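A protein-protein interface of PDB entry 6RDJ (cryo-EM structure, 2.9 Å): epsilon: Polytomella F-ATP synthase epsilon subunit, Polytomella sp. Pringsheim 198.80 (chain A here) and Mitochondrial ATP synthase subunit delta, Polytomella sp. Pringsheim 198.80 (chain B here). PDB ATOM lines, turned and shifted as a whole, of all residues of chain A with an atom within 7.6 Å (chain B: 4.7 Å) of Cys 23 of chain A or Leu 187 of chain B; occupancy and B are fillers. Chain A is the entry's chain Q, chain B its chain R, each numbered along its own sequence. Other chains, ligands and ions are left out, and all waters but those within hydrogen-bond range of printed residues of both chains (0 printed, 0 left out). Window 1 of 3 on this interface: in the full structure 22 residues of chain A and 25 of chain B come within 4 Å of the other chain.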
ATOM      1  N   PHE A   8      -5.110  -3.031 -17.094  1.00  0.00           N
ATOM      2  CA  PHE A   8      -6.032  -1.899 -17.147  1.00  0.00           C
ATOM      3  C   PHE A   8      -5.459  -0.648 -16.497  1.00  0.00           C
ATOM      4  O   PHE A   8      -5.856   0.465 -16.853  1.00  0.00           O
ATOM      5  CB  PHE A   8      -7.369  -2.270 -16.504  1.00  0.00           C
ATOM      6  CG  PHE A   8      -7.307  -2.496 -15.021  1.00  0.00           C
ATOM      7  CD1 PHE A   8      -7.666  -1.493 -14.135  1.00  0.00           C
ATOM      8  CD2 PHE A   8      -6.942  -3.725 -14.512  1.00  0.00           C
ATOM      9  CE1 PHE A   8      -7.619  -1.702 -12.780  1.00  0.00           C
ATOM     10  CE2 PHE A   8      -6.899  -3.940 -13.156  1.00  0.00           C
ATOM     11  CZ  PHE A   8      -7.242  -2.928 -12.291  1.00  0.00           C
ATOM     12  N   TYR A   9      -4.542  -0.802 -15.548  1.00  0.00           N
ATOM     13  CA  TYR A   9      -3.843   0.367 -15.036  1.00  0.00           C
ATOM     14  C   TYR A   9      -2.851   0.899 -16.055  1.00  0.00           C
ATOM     15  O   TYR A   9      -2.663   2.112 -16.158  1.00  0.00           O
ATOM     16  CB  TYR A   9      -3.141   0.037 -13.721  1.00  0.00           C
ATOM     17  CG  TYR A   9      -2.384  -1.266 -13.702  1.00  0.00           C
ATOM     18  CD1 TYR A   9      -2.975  -2.422 -13.224  1.00  0.00           C
ATOM     19  CD2 TYR A   9      -1.070  -1.331 -14.130  1.00  0.00           C
ATOM     20  CE1 TYR A   9      -2.288  -3.604 -13.196  1.00  0.00           C
ATOM     21  CE2 TYR A   9      -0.377  -2.511 -14.105  1.00  0.00           C
ATOM     22  CZ  TYR A   9      -0.991  -3.642 -13.637  1.00  0.00           C
ATOM     23  OH  TYR A   9      -0.304  -4.826 -13.610  1.00  0.00           O
ATOM     24  N   TYR A  16       2.483   0.743 -12.432  1.00  0.00           N
ATOM     25  CA  TYR A  16       2.133  -0.342 -11.529  1.00  0.00           C
ATOM     26  C   TYR A  16       2.295   0.086 -10.082  1.00  0.00           C
ATOM     27  O   TYR A  16       1.519  -0.334  -9.218  1.00  0.00           O
ATOM     28  CB  TYR A  16       2.974  -1.580 -11.797  1.00  0.00           C
ATOM     29  CG  TYR A  16       2.700  -2.648 -10.780  1.00  0.00           C
ATOM     30  CD1 TYR A  16       1.465  -3.265 -10.723  1.00  0.00           C
ATOM     31  CD2 TYR A  16       3.649  -3.001  -9.840  1.00  0.00           C
ATOM     32  CE1 TYR A  16       1.194  -4.222  -9.787  1.00  0.00           C
ATOM     33  CE2 TYR A  16       3.384  -3.951  -8.897  1.00  0.00           C
ATOM     34  CZ  TYR A  16       2.157  -4.560  -8.878  1.00  0.00           C
ATOM     35  OH  TYR A  16       1.894  -5.519  -7.938  1.00  0.00           O
ATOM     36  N   LEU A  17       3.302   0.915  -9.806  1.00  0.00           N
ATOM     37  CA  LEU A  17       3.544   1.387  -8.448  1.00  0.00           C
ATOM     38  C   LEU A  17       2.380   2.204  -7.929  1.00  0.00           C
ATOM     39  O   LEU A  17       1.948   2.018  -6.788  1.00  0.00           O
ATOM     40  CB  LEU A  17       4.811   2.225  -8.408  1.00  0.00           C
ATOM     41  CG  LEU A  17       6.115   1.460  -8.411  1.00  0.00           C
ATOM     42  CD1 LEU A  17       7.182   2.455  -8.660  1.00  0.00           C
ATOM     43  CD2 LEU A  17       6.302   0.803  -7.074  1.00  0.00           C
ATOM     44  N   ARG A  18       1.839   3.090  -8.763  1.00  0.00           N
ATOM     45  CA  ARG A  18       0.734   3.920  -8.317  1.00  0.00           C
ATOM     46  C   ARG A  18      -0.531   3.103  -8.150  1.00  0.00           C
ATOM     47  O   ARG A  18      -1.301   3.340  -7.219  1.00  0.00           O
ATOM     48  CB  ARG A  18       0.494   5.063  -9.288  1.00  0.00           C
ATOM     49  CG  ARG A  18      -0.378   6.124  -8.681  1.00  0.00           C
ATOM     50  CD  ARG A  18      -0.630   7.232  -9.642  1.00  0.00           C
ATOM     51  NE  ARG A  18       0.549   8.026  -9.929  1.00  0.00           N
ATOM     52  CZ  ARG A  18       0.890   9.100  -9.237  1.00  0.00           C
ATOM     53  NH1 ARG A  18       0.136   9.495  -8.224  1.00  0.00           N
ATOM     54  NH2 ARG A  18       1.977   9.782  -9.559  1.00  0.00           N
ATOM     55  N   TYR A  19      -0.734   2.107  -9.013  1.00  0.00           N
ATOM     56  CA  TYR A  19      -1.898   1.234  -8.896  1.00  0.00           C
ATOM     57  C   TYR A  19      -1.838   0.402  -7.624  1.00  0.00           C
ATOM     58  O   TYR A  19      -2.816   0.326  -6.868  1.00  0.00           O
ATOM     59  CB  TYR A  19      -1.986   0.335 -10.127  1.00  0.00           C
ATOM     60  CG  TYR A  19      -2.709  -0.966  -9.894  1.00  0.00           C
ATOM     61  CD1 TYR A  19      -2.012  -2.163  -9.782  1.00  0.00           C
ATOM     62  CD2 TYR A  19      -4.088  -1.000  -9.795  1.00  0.00           C
ATOM     63  CE1 TYR A  19      -2.667  -3.345  -9.564  1.00  0.00           C
ATOM     64  CE2 TYR A  19      -4.750  -2.178  -9.586  1.00  0.00           C
ATOM     65  CZ  TYR A  19      -4.037  -3.346  -9.467  1.00  0.00           C
ATOM     66  OH  TYR A  19      -4.695  -4.533  -9.253  1.00  0.00           O
ATOM     67  N   SER A  20      -0.686  -0.213  -7.366  1.00  0.00           N
ATOM     68  CA  SER A  20      -0.540  -1.058  -6.193  1.00  0.00           C
ATOM     69  C   SER A  20      -0.557  -0.242  -4.915  1.00  0.00           C
ATOM     70  O   SER A  20      -1.040  -0.720  -3.886  1.00  0.00           O
ATOM     71  CB  SER A  20       0.746  -1.863  -6.299  1.00  0.00           C
ATOM     72  OG  SER A  20       0.737  -2.929  -5.374  1.00  0.00           O
ATOM     73  N   ASN A  21      -0.090   1.004  -4.964  1.00  0.00           N
ATOM     74  CA  ASN A  21      -0.171   1.845  -3.782  1.00  0.00           C
ATOM     75  C   ASN A  21      -1.563   2.415  -3.584  1.00  0.00           C
ATOM     76  O   ASN A  21      -1.949   2.680  -2.445  1.00  0.00           O
ATOM     77  CB  ASN A  21       0.860   2.958  -3.860  1.00  0.00           C
ATOM     78  CG  ASN A  21       2.200   2.523  -3.346  1.00  0.00           C
ATOM     79  OD1 ASN A  21       2.409   2.439  -2.141  1.00  0.00           O
ATOM     80  ND2 ASN A  21       3.115   2.231  -4.251  1.00  0.00           N
ATOM     81  N   ILE A  22      -2.330   2.591  -4.661  1.00  0.00           N
ATOM     82  CA  ILE A  22      -3.747   2.916  -4.530  1.00  0.00           C
ATOM     83  C   ILE A  22      -4.486   1.781  -3.842  1.00  0.00           C
ATOM     84  O   ILE A  22      -5.279   2.009  -2.924  1.00  0.00           O
ATOM     85  CB  ILE A  22      -4.339   3.250  -5.912  1.00  0.00           C
ATOM     86  CG1 ILE A  22      -4.057   4.705  -6.267  1.00  0.00           C
ATOM     87  CG2 ILE A  22      -5.831   3.000  -5.964  1.00  0.00           C
ATOM     88  CD1 ILE A  22      -4.287   5.023  -7.709  1.00  0.00           C
ATOM     89  N   CYS A  23      -4.203   0.537  -4.239  1.00  0.00           N
ATOM     90  CA  CYS A  23      -4.829  -0.597  -3.562  1.00  0.00           C
ATOM     91  C   CYS A  23      -4.337  -0.752  -2.128  1.00  0.00           C
ATOM     92  O   CYS A  23      -5.110  -1.169  -1.260  1.00  0.00           O
ATOM     93  CB  CYS A  23      -4.603  -1.897  -4.329  1.00  0.00           C
ATOM     94  SG  CYS A  23      -5.056  -1.868  -6.054  1.00  0.00           S
ATOM     95  N   ALA A  24      -3.080  -0.416  -1.851  1.00  0.00           N
ATOM     96  CA  ALA A  24      -2.586  -0.481  -0.478  1.00  0.00           C
ATOM     97  C   ALA A  24      -3.257   0.568   0.400  1.00  0.00           C
ATOM     98  O   ALA A  24      -3.698   0.265   1.515  1.00  0.00           O
ATOM     99  CB  ALA A  24      -1.072  -0.307  -0.460  1.00  0.00           C
ATOM    100  N   ASP A  25      -3.369   1.802  -0.101  1.00  0.00           N
ATOM    101  CA  ASP A  25      -4.047   2.859   0.639  1.00  0.00           C
ATOM    102  C   ASP A  25      -5.531   2.565   0.794  1.00  0.00           C
ATOM    103  O   ASP A  25      -6.139   2.955   1.792  1.00  0.00           O
ATOM    104  CB  ASP A  25      -3.858   4.206  -0.059  1.00  0.00           C
ATOM    105  CG  ASP A  25      -2.406   4.653  -0.086  1.00  0.00           C
ATOM    106  OD1 ASP A  25      -1.628   4.219   0.786  1.00  0.00           O
ATOM    107  OD2 ASP A  25      -2.042   5.442  -0.982  1.00  0.00           O
ATOM    108  N   LEU A  26      -6.113   1.844  -0.153  1.00  0.00           N
ATOM    109  CA  LEU A  26      -7.520   1.495  -0.055  1.00  0.00           C
ATOM    110  C   LEU A  26      -7.755   0.348   0.913  1.00  0.00           C
ATOM    111  O   LEU A  26      -8.816   0.287   1.537  1.00  0.00           O
ATOM    112  CB  LEU A  26      -8.045   1.157  -1.443  1.00  0.00           C
ATOM    113  CG  LEU A  26      -8.833   2.200  -2.211  1.00  0.00           C
ATOM    114  CD1 LEU A  26      -8.195   3.547  -2.109  1.00  0.00           C
ATOM    115  CD2 LEU A  26      -8.817   1.779  -3.640  1.00  0.00           C
ATOM    116  N   LEU A  27      -6.794  -0.565   1.047  1.00  0.00           N
ATOM    117  CA  LEU A  27      -6.863  -1.528   2.139  1.00  0.00           C
ATOM    118  C   LEU A  27      -6.679  -0.843   3.484  1.00  0.00           C
ATOM    119  O   LEU A  27      -7.293  -1.250   4.474  1.00  0.00           O
ATOM    120  CB  LEU A  27      -5.816  -2.621   1.958  1.00  0.00           C
ATOM    121  CG  LEU A  27      -5.816  -3.747   2.990  1.00  0.00           C
ATOM    122  CD1 LEU A  27      -7.203  -4.318   3.127  1.00  0.00           C
ATOM    123  CD2 LEU A  27      -4.846  -4.838   2.635  1.00  0.00           C
ATOM    124  N   ARG A  28      -5.855   0.202   3.539  1.00  0.00           N
ATOM    125  CA  ARG A  28      -5.672   0.916   4.797  1.00  0.00           C
ATOM    126  C   ARG A  28      -6.885   1.760   5.172  1.00  0.00           C
ATOM    127  O   ARG A  28      -7.189   1.900   6.359  1.00  0.00           O
ATOM    128  CB  ARG A  28      -4.429   1.801   4.722  1.00  0.00           C
ATOM    129  CG  ARG A  28      -3.134   1.036   4.641  1.00  0.00           C
ATOM    130  CD  ARG A  28      -1.957   1.978   4.631  1.00  0.00           C
ATOM    131  NE  ARG A  28      -0.758   1.320   4.139  1.00  0.00           N
ATOM    132  CZ  ARG A  28      -0.176   1.616   2.986  1.00  0.00           C
ATOM    133  NH1 ARG A  28      -0.680   2.564   2.217  1.00  0.00           N
ATOM    134  NH2 ARG A  28       0.911   0.965   2.606  1.00  0.00           N
ATOM    135  N   ASN A  29      -7.597   2.313   4.193  1.00  0.00           N
ATOM    136  CA  ASN A  29      -8.718   3.202   4.472  1.00  0.00           C
ATOM    137  C   ASN A  29      -9.968   2.485   4.963  1.00  0.00           C
ATOM    138  O   ASN A  29     -10.960   3.154   5.262  1.00  0.00           O
ATOM    139  CB  ASN A  29      -9.076   4.012   3.222  1.00  0.00           C
ATOM    140  CG  ASN A  29      -8.140   5.175   2.991  1.00  0.00           C
ATOM    141  OD1 ASN A  29      -7.724   5.435   1.864  1.00  0.00           O
ATOM    142  ND2 ASN A  29      -7.802   5.885   4.060  1.00  0.00           N
ATOM    143  N   VAL A  30      -9.971   1.152   5.019  1.00  0.00           N
ATOM    144  CA  VAL A  30     -11.082   0.396   5.589  1.00  0.00           C
ATOM    145  C   VAL A  30     -10.539  -0.563   6.635  1.00  0.00           C
ATOM    146  O   VAL A  30     -11.163  -1.579   6.960  1.00  0.00           O
ATOM    147  CB  VAL A  30     -11.885  -0.356   4.510  1.00  0.00           C
ATOM    148  CG1 VAL A  30     -12.555   0.623   3.564  1.00  0.00           C
ATOM    149  CG2 VAL A  30     -10.980  -1.290   3.727  1.00  0.00           C
ATOM    150  N   ILE A  69      -1.242   8.244  -1.688  1.00  0.00           N
ATOM    151  CA  ILE A  69      -0.778   8.513  -3.042  1.00  0.00           C
ATOM    152  C   ILE A  69      -1.960   9.139  -3.779  1.00  0.00           C
ATOM    153  O   ILE A  69      -3.114   8.893  -3.392  1.00  0.00           O
ATOM    154  CB  ILE A  69      -0.232   7.215  -3.680  1.00  0.00           C
ATOM    155  CG1 ILE A  69       0.805   7.489  -4.768  1.00  0.00           C
ATOM    156  CG2 ILE A  69      -1.340   6.338  -4.219  1.00  0.00           C
ATOM    157  CD1 ILE A  69       1.707   6.328  -5.063  1.00  0.00           C
ATOM    158  N   PRO B 113      -5.897  -8.847  -5.348  1.00  0.00           N
ATOM    159  CA  PRO B 113      -6.330  -8.689  -3.954  1.00  0.00           C
ATOM    160  C   PRO B 113      -7.090  -9.885  -3.411  1.00  0.00           C
ATOM    161  O   PRO B 113      -8.190 -10.195  -3.872  1.00  0.00           O
ATOM    162  CB  PRO B 113      -7.232  -7.458  -4.024  1.00  0.00           C
ATOM    163  CG  PRO B 113      -6.631  -6.649  -5.072  1.00  0.00           C
ATOM    164  CD  PRO B 113      -6.040  -7.584  -6.088  1.00  0.00           C
ATOM    165  N   PHE B 128      -4.852 -11.281   4.358  1.00  0.00           N
ATOM    166  CA  PHE B 128      -5.436 -10.624   3.200  1.00  0.00           C
ATOM    167  C   PHE B 128      -4.433  -9.623   2.645  1.00  0.00           C
ATOM    168  O   PHE B 128      -4.133  -8.620   3.293  1.00  0.00           O
ATOM    169  CB  PHE B 128      -6.737  -9.918   3.562  1.00  0.00           C
ATOM    170  CG  PHE B 128      -7.392  -9.238   2.402  1.00  0.00           C
ATOM    171  CD1 PHE B 128      -8.130  -9.965   1.493  1.00  0.00           C
ATOM    172  CD2 PHE B 128      -7.269  -7.874   2.216  1.00  0.00           C
ATOM    173  CE1 PHE B 128      -8.730  -9.348   0.421  1.00  0.00           C
ATOM    174  CE2 PHE B 128      -7.863  -7.257   1.141  1.00  0.00           C
ATOM    175  CZ  PHE B 128      -8.596  -7.993   0.247  1.00  0.00           C
ATOM    176  N   SER B 130      -3.176  -6.965  -0.536  1.00  0.00           N
ATOM    177  CA  SER B 130      -3.832  -6.015  -1.416  1.00  0.00           C
ATOM    178  C   SER B 130      -3.321  -6.088  -2.844  1.00  0.00           C
ATOM    179  O   SER B 130      -3.583  -5.177  -3.633  1.00  0.00           O
ATOM    180  CB  SER B 130      -3.662  -4.604  -0.881  1.00  0.00           C
ATOM    181  OG  SER B 130      -4.507  -3.739  -1.594  1.00  0.00           O
ATOM    182  N   ALA B 183      -9.985  -0.823  -9.459  1.00  0.00           N
ATOM    183  CA  ALA B 183      -9.164  -1.388  -8.392  1.00  0.00           C
ATOM    184  C   ALA B 183      -9.878  -1.318  -7.052  1.00  0.00           C
ATOM    185  O   ALA B 183      -9.818  -2.265  -6.259  1.00  0.00           O
ATOM    186  CB  ALA B 183      -7.828  -0.658  -8.320  1.00  0.00           C
ATOM    187  N   ALA B 184     -10.605  -0.221  -6.817  1.00  0.00           N
ATOM    188  CA  ALA B 184     -11.377  -0.057  -5.591  1.00  0.00           C
ATOM    189  C   ALA B 184     -12.469  -1.105  -5.472  1.00  0.00           C
ATOM    190  O   ALA B 184     -12.606  -1.751  -4.427  1.00  0.00           O
ATOM    191  CB  ALA B 184     -11.984   1.343  -5.548  1.00  0.00           C
ATOM    192  N   ILE B 185     -13.255  -1.291  -6.536  1.00  0.00           N
ATOM    193  CA  ILE B 185     -14.387  -2.202  -6.436  1.00  0.00           C
ATOM    194  C   ILE B 185     -13.915  -3.645  -6.382  1.00  0.00           C
ATOM    195  O   ILE B 185     -14.485  -4.452  -5.645  1.00  0.00           O
ATOM    196  CB  ILE B 185     -15.418  -1.973  -7.561  1.00  0.00           C
ATOM    197  CG1 ILE B 185     -14.835  -2.215  -8.951  1.00  0.00           C
ATOM    198  CG2 ILE B 185     -16.004  -0.587  -7.466  1.00  0.00           C
ATOM    199  CD1 ILE B 185     -15.874  -2.271 -10.034  1.00  0.00           C
ATOM    200  N   GLU B 186     -12.814  -3.977  -7.071  1.00  0.00           N
ATOM    201  CA  GLU B 186     -12.352  -5.357  -7.001  1.00  0.00           C
ATOM    202  C   GLU B 186     -11.696  -5.652  -5.657  1.00  0.00           C
ATOM    203  O   GLU B 186     -11.898  -6.742  -5.110  1.00  0.00           O
ATOM    204  CB  GLU B 186     -11.432  -5.685  -8.184  1.00  0.00           C
ATOM    205  CG  GLU B 186      -9.996  -5.223  -8.099  1.00  0.00           C
ATOM    206  CD  GLU B 186      -9.109  -5.922  -9.104  1.00  0.00           C
ATOM    207  OE1 GLU B 186      -7.875  -5.913  -8.921  1.00  0.00           O
ATOM    208  OE2 GLU B 186      -9.645  -6.487 -10.077  1.00  0.00           O
ATOM    209  N   LEU B 187     -11.028  -4.664  -5.052  1.00  0.00           N
ATOM    210  CA  LEU B 187     -10.408  -4.893  -3.755  1.00  0.00           C
ATOM    211  C   LEU B 187     -11.456  -4.999  -2.657  1.00  0.00           C
ATOM    212  O   LEU B 187     -11.433  -5.942  -1.859  1.00  0.00           O
ATOM    213  CB  LEU B 187      -9.414  -3.776  -3.450  1.00  0.00           C
ATOM    214  CG  LEU B 187      -8.953  -3.662  -2.004  1.00  0.00           C
ATOM    215  CD1 LEU B 187      -8.130  -4.851  -1.582  1.00  0.00           C
ATOM    216  CD2 LEU B 187      -8.144  -2.434  -1.878  1.00  0.00           C
ATOM    217  N   TYR B 188     -12.397  -4.052  -2.614  1.00  0.00           N
ATOM    218  CA  TYR B 188     -13.423  -4.091  -1.581  1.00  0.00           C
ATOM    219  C   TYR B 188     -14.376  -5.260  -1.777  1.00  0.00           C
ATOM    220  O   TYR B 188     -14.858  -5.824  -0.791  1.00  0.00           O
ATOM    221  CB  TYR B 188     -14.206  -2.784  -1.565  1.00  0.00           C
ATOM    222  CG  TYR B 188     -13.426  -1.569  -1.138  1.00  0.00           C
ATOM    223  CD1 TYR B 188     -12.475  -1.643  -0.130  1.00  0.00           C
ATOM    224  CD2 TYR B 188     -13.644  -0.343  -1.748  1.00  0.00           C
ATOM    225  CE1 TYR B 188     -11.766  -0.524   0.251  1.00  0.00           C
ATOM    226  CE2 TYR B 188     -12.941   0.775  -1.377  1.00  0.00           C
ATOM    227  CZ  TYR B 188     -12.010   0.682  -0.375  1.00  0.00           C
ATOM    228  OH  TYR B 188     -11.316   1.809  -0.008  1.00  0.00           O
ATOM    229  N   SER B 189     -14.628  -5.671  -3.027  1.00  0.00           N
ATOM    230  CA  SER B 189     -15.493  -6.818  -3.264  1.00  0.00           C
ATOM    231  C   SER B 189     -14.813  -8.116  -2.862  1.00  0.00           C
ATOM    232  O   SER B 189     -15.460  -9.003  -2.296  1.00  0.00           O
ATOM    233  CB  SER B 189     -15.908  -6.865  -4.729  1.00  0.00           C
ATOM    234  OG  SER B 189     -14.787  -7.095  -5.555  1.00  0.00           O
ATOM    235  N   ALA B 190     -13.506  -8.244  -3.119  1.00  0.00           N
ATOM    236  CA  ALA B 190     -12.789  -9.413  -2.624  1.00  0.00           C
ATOM    237  C   ALA B 190     -12.685  -9.400  -1.107  1.00  0.00           C
ATOM    238  O   ALA B 190     -12.689 -10.462  -0.473  1.00  0.00           O
ATOM    239  CB  ALA B 190     -11.400  -9.488  -3.249  1.00  0.00           C
ATOM    240  N   LEU B 191     -12.646  -8.208  -0.513  1.00  0.00           N
ATOM    241  CA  LEU B 191     -12.569  -8.105   0.937  1.00  0.00           C
ATOM    242  C   LEU B 191     -13.886  -8.496   1.594  1.00  0.00           C
ATOM    243  O   LEU B 191     -13.887  -9.177   2.624  1.00  0.00           O
ATOM    244  CB  LEU B 191     -12.160  -6.689   1.322  1.00  0.00           C
ATOM    245  CG  LEU B 191     -11.710  -6.442   2.751  1.00  0.00           C
ATOM    246  CD1 LEU B 191     -10.825  -7.572   3.259  1.00  0.00           C
ATOM    247  CD2 LEU B 191     -10.969  -5.134   2.767  1.00  0.00           C
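Ala 183 of chain B touches Tyr 19 of chain A (CB to CE2, 3.7 Å). Leu 187 of chain B touches Cys 23 of chain A (CD2 to O, 3.3 Å). N of Ala 24 of chain A touches OG of Ser 130 of chain B, 3.6 Å away. CD2 of Leu 187 of chain B touches CB of Leu 26 of chain A (3.6 Å). CE2 of Phe 128 of chain B touches CD1 of Leu 27 of chain A (3.6 Å). Ser 130 of chain B touches Leu 27 of chain A. CD2 of Leu 187 of chain B touches N of Leu 27 of chain A, at 3.7 Å. CD1 of Leu 27 of chain A touches CD2 of Leu 191 of chain B (3.9 Å). Val 30 of chain A touches Tyr 188 of chain B (CG1 to CE1, 3.6 Å). Val 30 of chain A touches Leu 191 of chain B.
Of chain B, only Ser 130, Ala 183 and Leu 187 come within 4 Å of Cys 23 of chain A. Of the printed residues of chain B, Ala 24 of chain A touches Ser 130 (3.6 Å). Printed residues of chain B within 4 Å of Leu 27 of chain A: Phe 128, Ser 130, Leu 187 and Leu 191. Printed residues of chain B within 4 Å of Val 30 of chain A: Tyr 188 (3.6 Å) and Leu 191 (3.96 Å). Of the printed residues of chain A, Ala 183 of chain B touches Tyr 19 and Cys 23. Ile 185 of chain B touches none of the printed residues of chain A. Of the printed residues of chain A, Leu 191 of chain B touches Leu 27 and Val 30. The nearest printed residue of chain A that does not touch Ser 130 of chain B is Ser 20 of chain A (5.1 Å).
The backbone carbonyl oxygen of Leu 26 of chain A lies within hydrogen-bond range of the side-chain hydroxyl of Tyr 188 of chain B. The side-chain hydroxyl (OH) of Tyr 19 of chain A lies within hydrogen-bond range of the side-chain carboxylate (OE1) of Glu 186 of chain B (3.5 Å). The backbone carbonyl oxygen of Cys 23 of chain A sits at hydrogen-bond distance from the side-chain hydroxyl of Ser 130 of chain B.
O of Glu 186 of chain B lies within hydrogen-bond range of OG of Ser 189 of chain B. The side-chain sulfur (SG) of Cys 23 of chain A sits at hydrogen-bond distance from the backbone carbonyl oxygen (O) of Tyr 19 of chain A, 3.2 Å away.
Printed residues of chain B that touch a printed residue of chain A: Phe 128, Ser 130, Ala 183, Ala 184, Glu 186, Leu 187, Tyr 188 and Leu 191. Of the 18 printed residues of chain A, 6 touch a printed residue of chain B. Hydrophobic or aromatic side chains of chain A within 4 Å of the printed part of chain B: Tyr 19, Leu 26, Leu 27 and Val 30. Among the printed residues, no Asp or Glu carboxylate lies within 4 Å of a Lys or Arg side-chain nitrogen of the other chain.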
